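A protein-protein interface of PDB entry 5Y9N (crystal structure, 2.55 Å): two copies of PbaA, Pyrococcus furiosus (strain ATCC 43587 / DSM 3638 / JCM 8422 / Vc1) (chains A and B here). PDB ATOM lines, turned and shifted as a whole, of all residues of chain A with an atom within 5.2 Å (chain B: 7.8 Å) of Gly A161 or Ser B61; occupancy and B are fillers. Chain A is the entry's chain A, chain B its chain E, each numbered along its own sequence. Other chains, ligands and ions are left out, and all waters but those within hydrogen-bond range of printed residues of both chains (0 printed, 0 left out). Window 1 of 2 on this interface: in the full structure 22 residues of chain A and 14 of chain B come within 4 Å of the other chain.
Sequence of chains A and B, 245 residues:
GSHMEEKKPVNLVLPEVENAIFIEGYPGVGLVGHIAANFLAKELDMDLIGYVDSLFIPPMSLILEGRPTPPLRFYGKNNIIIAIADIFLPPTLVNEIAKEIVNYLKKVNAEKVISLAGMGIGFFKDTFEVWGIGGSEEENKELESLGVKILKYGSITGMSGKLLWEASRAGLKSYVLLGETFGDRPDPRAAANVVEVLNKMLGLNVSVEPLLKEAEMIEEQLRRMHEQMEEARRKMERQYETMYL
The backbone carbonyl oxygen (O) of Gly A154 sits at hydrogen-bond distance from the backbone NH (N) of Ile B63 (2.7 Å).
The backbone carbonyl oxygen (O) of Ile A156 lies within hydrogen-bond range of the backbone NH (N) of Ser B61, at 2.8 Å.
The backbone carbonyl oxygen (O) of Pro B59 is in hydrogen-bond range of the backbone NH (N) of Gly A158 (3.0 Å).
The backbone carbonyl oxygen (O) of Gly A161 lies within hydrogen-bond range of the side-chain hydroxyl (OG) of Ser B61.
The backbone carbonyl oxygen (O) of Leu B62 is in hydrogen-bond range of the backbone NH (N) of Thr B69.
Ser B61 touches Ser A155.
O of Ile A156 touches CA of Met B60, at 3.1 Å.
Ile A156 touches Ile B63.
O of Pro B59 touches CA of Thr A157 (3.6 Å).
Thr A157 touches Met B60 (CA to CB, 3.9 Å).
O of Gly A161 touches C of Met B60 (3.9 Å).
Lys A162 touches Pro B59.
Leu A164 touches Pro B68.
Trp A165 touches Ser B61.
Pro B68 touches Trp A165 (O to CZ3, 3.5 Å).
Of the printed residues of chain B, Ile A156 touches Met B60 (3.1 Å), Ser B61 (2.8 Å) and Ile B63 (3.96 Å).
Printed residues of chain B within 4 Å of Trp A165: Ser B61, Pro B68 and Pro B70.
Ser B61 touches four residues of chain A.
Printed residues of chain A within 4 Å of Leu B62: Gly A154.
Of the printed residues of chain A, Ile B63 touches Gly A154 (2.7 Å) and Ile A156 (3.96 Å).
Leu B64 touches none of the printed residues of chain A.
Of the printed residues of chain A, Pro B68 touches Leu A164 (3.5 Å) and Trp A165 (3.5 Å).
Of the 12 printed residues of chain B, 7 touch a printed residue of chain A.
Hydrophobic or aromatic side chains of chain B that line the printed part of chain A: Pro B59, Met B60, Ile B63, Pro B68 and Pro B70.
Of the 12 printed residues of chain A, 9 touch a printed residue of chain B.
No position is printed for both chains.
Of the 16 pairs that touch across the chains among the printed residues, none has its exchanged pair printed and touching as well.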
ATOM      1  N   GLY A 154       9.050  16.295  23.442  1.00  0.00           N
ATOM      2  CA  GLY A 154      10.277  15.952  22.727  1.00  0.00           C
ATOM      3  C   GLY A 154      11.483  15.883  23.615  1.00  0.00           C
ATOM      4  O   GLY A 154      11.373  16.004  24.820  1.00  0.00           O
ATOM      5  N   SER A 155      12.624  15.592  23.019  1.00  0.00           N
ATOM      6  CA  SER A 155      13.894  15.699  23.717  1.00  0.00           C
ATOM      7  C   SER A 155      14.872  16.369  22.821  1.00  0.00           C
ATOM      8  O   SER A 155      14.808  16.254  21.604  1.00  0.00           O
ATOM      9  CB  SER A 155      14.434  14.354  24.149  1.00  0.00           C
ATOM     10  OG  SER A 155      14.539  13.517  23.052  1.00  0.00           O
ATOM     11  N   ILE A 156      15.734  17.140  23.452  1.00  0.00           N
ATOM     12  CA  ILE A 156      16.741  17.905  22.764  1.00  0.00           C
ATOM     13  C   ILE A 156      17.996  17.496  23.486  1.00  0.00           C
ATOM     14  O   ILE A 156      18.162  17.807  24.672  1.00  0.00           O
ATOM     15  CB  ILE A 156      16.496  19.402  22.889  1.00  0.00           C
ATOM     16  CG1 ILE A 156      15.112  19.749  22.333  1.00  0.00           C
ATOM     17  CG2 ILE A 156      17.616  20.169  22.203  1.00  0.00           C
ATOM     18  CD1 ILE A 156      14.702  21.171  22.544  1.00  0.00           C
ATOM     19  N   THR A 157      18.853  16.759  22.782  1.00  0.00           N
ATOM     20  CA  THR A 157      20.082  16.235  23.340  1.00  0.00           C
ATOM     21  C   THR A 157      21.228  17.160  23.008  1.00  0.00           C
ATOM     22  O   THR A 157      21.099  18.072  22.187  1.00  0.00           O
ATOM     23  CB  THR A 157      20.377  14.857  22.755  1.00  0.00           C
ATOM     24  OG1 THR A 157      20.326  14.943  21.332  1.00  0.00           O
ATOM     25  CG2 THR A 157      19.338  13.847  23.252  1.00  0.00           C
ATOM     26  N   GLY A 158      22.349  16.955  23.676  1.00  0.00           N
ATOM     27  CA  GLY A 158      23.536  17.718  23.344  1.00  0.00           C
ATOM     28  C   GLY A 158      23.545  19.079  23.983  1.00  0.00           C
ATOM     29  O   GLY A 158      22.746  19.372  24.886  1.00  0.00           O
ATOM     30  N   MET A 159      24.472  19.901  23.509  1.00  0.00           N
ATOM     31  CA  MET A 159      24.715  21.208  24.087  1.00  0.00           C
ATOM     32  C   MET A 159      23.432  22.044  24.165  1.00  0.00           C
ATOM     33  O   MET A 159      23.175  22.728  25.142  1.00  0.00           O
ATOM     34  CB  MET A 159      25.798  21.920  23.281  1.00  0.00           C
ATOM     35  CG  MET A 159      26.202  23.274  23.818  1.00  0.00           C
ATOM     36  SD  MET A 159      26.810  23.203  25.455  1.00  0.00           S
ATOM     37  CE  MET A 159      28.516  22.937  25.158  1.00  0.00           C
ATOM     38  N   SER A 160      22.634  21.981  23.118  1.00  0.00           N
ATOM     39  CA  SER A 160      21.402  22.748  23.029  1.00  0.00           C
ATOM     40  C   SER A 160      20.473  22.454  24.175  1.00  0.00           C
ATOM     41  O   SER A 160      20.030  23.362  24.867  1.00  0.00           O
ATOM     42  CB  SER A 160      20.720  22.496  21.704  1.00  0.00           C
ATOM     43  OG  SER A 160      21.551  23.025  20.701  1.00  0.00           O
ATOM     44  N   GLY A 161      20.215  21.178  24.376  1.00  0.00           N
ATOM     45  CA  GLY A 161      19.382  20.713  25.471  1.00  0.00           C
ATOM     46  C   GLY A 161      19.899  21.093  26.838  1.00  0.00           C
ATOM     47  O   GLY A 161      19.120  21.457  27.708  1.00  0.00           O
ATOM     48  N   LYS A 162      21.207  21.006  27.035  1.00  0.00           N
ATOM     49  CA  LYS A 162      21.785  21.324  28.318  1.00  0.00           C
ATOM     50  C   LYS A 162      21.714  22.831  28.562  1.00  0.00           C
ATOM     51  O   LYS A 162      21.326  23.250  29.643  1.00  0.00           O
ATOM     52  CB  LYS A 162      23.232  20.801  28.457  1.00  0.00           C
ATOM     53  CG  LYS A 162      23.730  20.751  29.911  1.00  0.00           C
ATOM     54  CD  LYS A 162      23.069  19.594  30.653  1.00  0.00           C
ATOM     55  CE  LYS A 162      23.074  19.688  32.161  1.00  0.00           C
ATOM     56  NZ  LYS A 162      24.416  19.399  32.656  1.00  0.00           N
ATOM     57  N   LEU A 163      22.093  23.634  27.575  1.00  0.00           N
ATOM     58  CA  LEU A 163      22.043  25.095  27.719  1.00  0.00           C
ATOM     59  C   LEU A 163      20.641  25.593  27.998  1.00  0.00           C
ATOM     60  O   LEU A 163      20.441  26.458  28.846  1.00  0.00           O
ATOM     61  CB  LEU A 163      22.534  25.788  26.472  1.00  0.00           C
ATOM     62  CG  LEU A 163      24.026  25.974  26.356  1.00  0.00           C
ATOM     63  CD1 LEU A 163      24.298  26.780  25.100  1.00  0.00           C
ATOM     64  CD2 LEU A 163      24.569  26.688  27.578  1.00  0.00           C
ATOM     65  N   LEU A 164      19.670  25.041  27.271  1.00  0.00           N
ATOM     66  CA  LEU A 164      18.291  25.407  27.469  1.00  0.00           C
ATOM     67  C   LEU A 164      17.929  25.337  28.959  1.00  0.00           C
ATOM     68  O   LEU A 164      17.448  26.301  29.533  1.00  0.00           O
ATOM     69  CB  LEU A 164      17.390  24.472  26.679  1.00  0.00           C
ATOM     70  CG  LEU A 164      15.878  24.698  26.859  1.00  0.00           C
ATOM     71  CD1 LEU A 164      15.517  26.103  26.393  1.00  0.00           C
ATOM     72  CD2 LEU A 164      15.103  23.630  26.119  1.00  0.00           C
ATOM     73  N   TRP A 165      18.187  24.189  29.572  1.00  0.00           N
ATOM     74  CA  TRP A 165      17.856  23.959  30.961  1.00  0.00           C
ATOM     75  C   TRP A 165      18.735  24.795  31.903  1.00  0.00           C
ATOM     76  O   TRP A 165      18.217  25.526  32.743  1.00  0.00           O
ATOM     77  CB  TRP A 165      17.978  22.472  31.296  1.00  0.00           C
ATOM     78  CG  TRP A 165      17.860  22.203  32.739  1.00  0.00           C
ATOM     79  CD1 TRP A 165      18.858  21.862  33.601  1.00  0.00           C
ATOM     80  CD2 TRP A 165      16.669  22.300  33.510  1.00  0.00           C
ATOM     81  NE1 TRP A 165      18.353  21.701  34.861  1.00  0.00           N
ATOM     82  CE2 TRP A 165      17.012  21.996  34.840  1.00  0.00           C
ATOM     83  CE3 TRP A 165      15.337  22.621  33.206  1.00  0.00           C
ATOM     84  CZ2 TRP A 165      16.062  21.985  35.871  1.00  0.00           C
ATOM     85  CZ3 TRP A 165      14.397  22.618  34.229  1.00  0.00           C
ATOM     86  CH2 TRP A 165      14.768  22.304  35.550  1.00  0.00           C
ATOM     87  N   PRO B  58      23.841  12.342  30.761  1.00  0.00           N
ATOM     88  CA  PRO B  58      24.123  12.906  29.464  1.00  0.00           C
ATOM     89  C   PRO B  58      23.288  14.142  29.192  1.00  0.00           C
ATOM     90  O   PRO B  58      22.153  14.200  29.614  1.00  0.00           O
ATOM     91  CB  PRO B  58      23.816  11.762  28.474  1.00  0.00           C
ATOM     92  CG  PRO B  58      23.124  10.723  29.228  1.00  0.00           C
ATOM     93  CD  PRO B  58      23.397  10.940  30.682  1.00  0.00           C
ATOM     94  N   PRO B  59      23.855  15.102  28.465  1.00  0.00           N
ATOM     95  CA  PRO B  59      23.201  16.381  28.207  1.00  0.00           C
ATOM     96  C   PRO B  59      21.931  16.212  27.413  1.00  0.00           C
ATOM     97  O   PRO B  59      21.963  15.668  26.319  1.00  0.00           O
ATOM     98  CB  PRO B  59      24.228  17.140  27.359  1.00  0.00           C
ATOM     99  CG  PRO B  59      25.043  16.078  26.686  1.00  0.00           C
ATOM    100  CD  PRO B  59      25.086  14.922  27.649  1.00  0.00           C
ATOM    101  N   MET B  60      20.820  16.662  27.981  1.00  0.00           N
ATOM    102  CA  MET B  60      19.549  16.759  27.264  1.00  0.00           C
ATOM    103  C   MET B  60      18.552  17.574  28.059  1.00  0.00           C
ATOM    104  O   MET B  60      18.717  17.755  29.264  1.00  0.00           O
ATOM    105  CB  MET B  60      18.941  15.379  27.005  1.00  0.00           C
ATOM    106  CG  MET B  60      18.499  14.642  28.251  1.00  0.00           C
ATOM    107  SD  MET B  60      18.505  12.845  28.018  1.00  0.00           S
ATOM    108  CE  MET B  60      16.996  12.644  27.093  1.00  0.00           C
ATOM    109  N   SER B  61      17.522  18.050  27.369  1.00  0.00           N
ATOM    110  CA  SER B  61      16.269  18.471  28.003  1.00  0.00           C
ATOM    111  C   SER B  61      15.166  17.659  27.377  1.00  0.00           C
ATOM    112  O   SER B  61      15.115  17.487  26.158  1.00  0.00           O
ATOM    113  CB  SER B  61      15.966  19.939  27.767  1.00  0.00           C
ATOM    114  OG  SER B  61      16.720  20.749  28.624  1.00  0.00           O
ATOM    115  N   LEU B  62      14.284  17.176  28.232  1.00  0.00           N
ATOM    116  CA  LEU B  62      13.008  16.669  27.798  1.00  0.00           C
ATOM    117  C   LEU B  62      12.074  17.861  27.747  1.00  0.00           C
ATOM    118  O   LEU B  62      12.189  18.776  28.556  1.00  0.00           O
ATOM    119  CB  LEU B  62      12.476  15.695  28.808  1.00  0.00           C
ATOM    120  CG  LEU B  62      13.402  14.539  29.176  1.00  0.00           C
ATOM    121  CD1 LEU B  62      12.767  13.852  30.363  1.00  0.00           C
ATOM    122  CD2 LEU B  62      13.600  13.566  28.033  1.00  0.00           C
ATOM    123  N   ILE B  63      11.152  17.853  26.804  1.00  0.00           N
ATOM    124  CA  ILE B  63      10.156  18.885  26.701  1.00  0.00           C
ATOM    125  C   ILE B  63       8.837  18.220  27.047  1.00  0.00           C
ATOM    126  O   ILE B  63       8.440  17.273  26.367  1.00  0.00           O
ATOM    127  CB  ILE B  63      10.095  19.456  25.271  1.00  0.00           C
ATOM    128  CG1 ILE B  63      11.493  19.841  24.757  1.00  0.00           C
ATOM    129  CG2 ILE B  63       9.156  20.645  25.199  1.00  0.00           C
ATOM    130  CD1 ILE B  63      12.240  20.806  25.624  1.00  0.00           C
ATOM    131  N   LEU B  64       8.176  18.700  28.103  1.00  0.00           N
ATOM    132  CA  LEU B  64       6.854  18.185  28.535  1.00  0.00           C
ATOM    133  C   LEU B  64       5.863  19.330  28.668  1.00  0.00           C
ATOM    134  O   LEU B  64       6.096  20.250  29.451  1.00  0.00           O
ATOM    135  CB  LEU B  64       6.988  17.464  29.875  1.00  0.00           C
ATOM    136  CG  LEU B  64       8.074  16.379  29.936  1.00  0.00           C
ATOM    137  CD1 LEU B  64       8.429  15.978  31.336  1.00  0.00           C
ATOM    138  CD2 LEU B  64       7.662  15.147  29.132  1.00  0.00           C
ATOM    139  N   ARG B  67       7.486  22.720  28.418  1.00  0.00           N
ATOM    140  CA  ARG B  67       8.466  23.134  29.417  1.00  0.00           C
ATOM    141  C   ARG B  67       9.695  22.222  29.412  1.00  0.00           C
ATOM    142  O   ARG B  67       9.565  21.012  29.511  1.00  0.00           O
ATOM    143  CB  ARG B  67       7.835  23.214  30.825  1.00  0.00           C
ATOM    144  CG  ARG B  67       7.639  24.674  31.299  1.00  0.00           C
ATOM    145  CD  ARG B  67       6.432  24.880  32.194  1.00  0.00           C
ATOM    146  NE  ARG B  67       5.204  24.404  31.562  1.00  0.00           N
ATOM    147  CZ  ARG B  67       4.049  24.167  32.186  1.00  0.00           C
ATOM    148  NH1 ARG B  67       3.906  24.387  33.497  1.00  0.00           N
ATOM    149  NH2 ARG B  67       3.008  23.707  31.488  1.00  0.00           N
ATOM    150  N   PRO B  68      10.883  22.815  29.287  1.00  0.00           N
ATOM    151  CA  PRO B  68      12.106  22.037  29.436  1.00  0.00           C
ATOM    152  C   PRO B  68      12.190  21.411  30.807  1.00  0.00           C
ATOM    153  O   PRO B  68      12.008  22.112  31.784  1.00  0.00           O
ATOM    154  CB  PRO B  68      13.222  23.082  29.282  1.00  0.00           C
ATOM    155  CG  PRO B  68      12.603  24.205  28.540  1.00  0.00           C
ATOM    156  CD  PRO B  68      11.163  24.221  28.942  1.00  0.00           C
ATOM    157  N   THR B  69      12.429  20.103  30.876  1.00  0.00           N
ATOM    158  CA  THR B  69      12.677  19.433  32.160  1.00  0.00           C
ATOM    159  C   THR B  69      13.911  18.519  32.044  1.00  0.00           C
ATOM    160  O   THR B  69      14.202  18.027  30.964  1.00  0.00           O
ATOM    161  CB  THR B  69      11.446  18.623  32.637  1.00  0.00           C
ATOM    162  OG1 THR B  69      11.469  17.313  32.078  1.00  0.00           O
ATOM    163  CG2 THR B  69      10.149  19.279  32.197  1.00  0.00           C
ATOM    164  N   PRO B  70      14.648  18.295  33.146  1.00  0.00           N
ATOM    165  CA  PRO B  70      15.776  17.368  33.099  1.00  0.00           C
ATOM    166  C   PRO B  70      15.328  15.920  33.046  1.00  0.00           C
ATOM    167  O   PRO B  70      14.198  15.606  33.408  1.00  0.00           O
ATOM    168  CB  PRO B  70      16.491  17.583  34.435  1.00  0.00           C
ATOM    169  CG  PRO B  70      15.861  18.767  35.044  1.00  0.00           C
ATOM    170  CD  PRO B  70      14.478  18.832  34.506  1.00  0.00           C
ATOM    171  N   PRO B  71      16.229  15.031  32.618  1.00  0.00           N
ATOM    172  CA  PRO B  71      15.863  13.630  32.466  1.00  0.00           C
ATOM    173  C   PRO B  71      15.582  12.879  33.766  1.00  0.00           C
ATOM    174  O   PRO B  71      14.847  11.894  33.740  1.00  0.00           O
ATOM    175  CB  PRO B  71      17.077  13.025  31.750  1.00  0.00           C
ATOM    176  CG  PRO B  71      18.190  13.951  32.047  1.00  0.00           C
ATOM    177  CD  PRO B  71      17.577  15.305  32.113  1.00  0.00           C
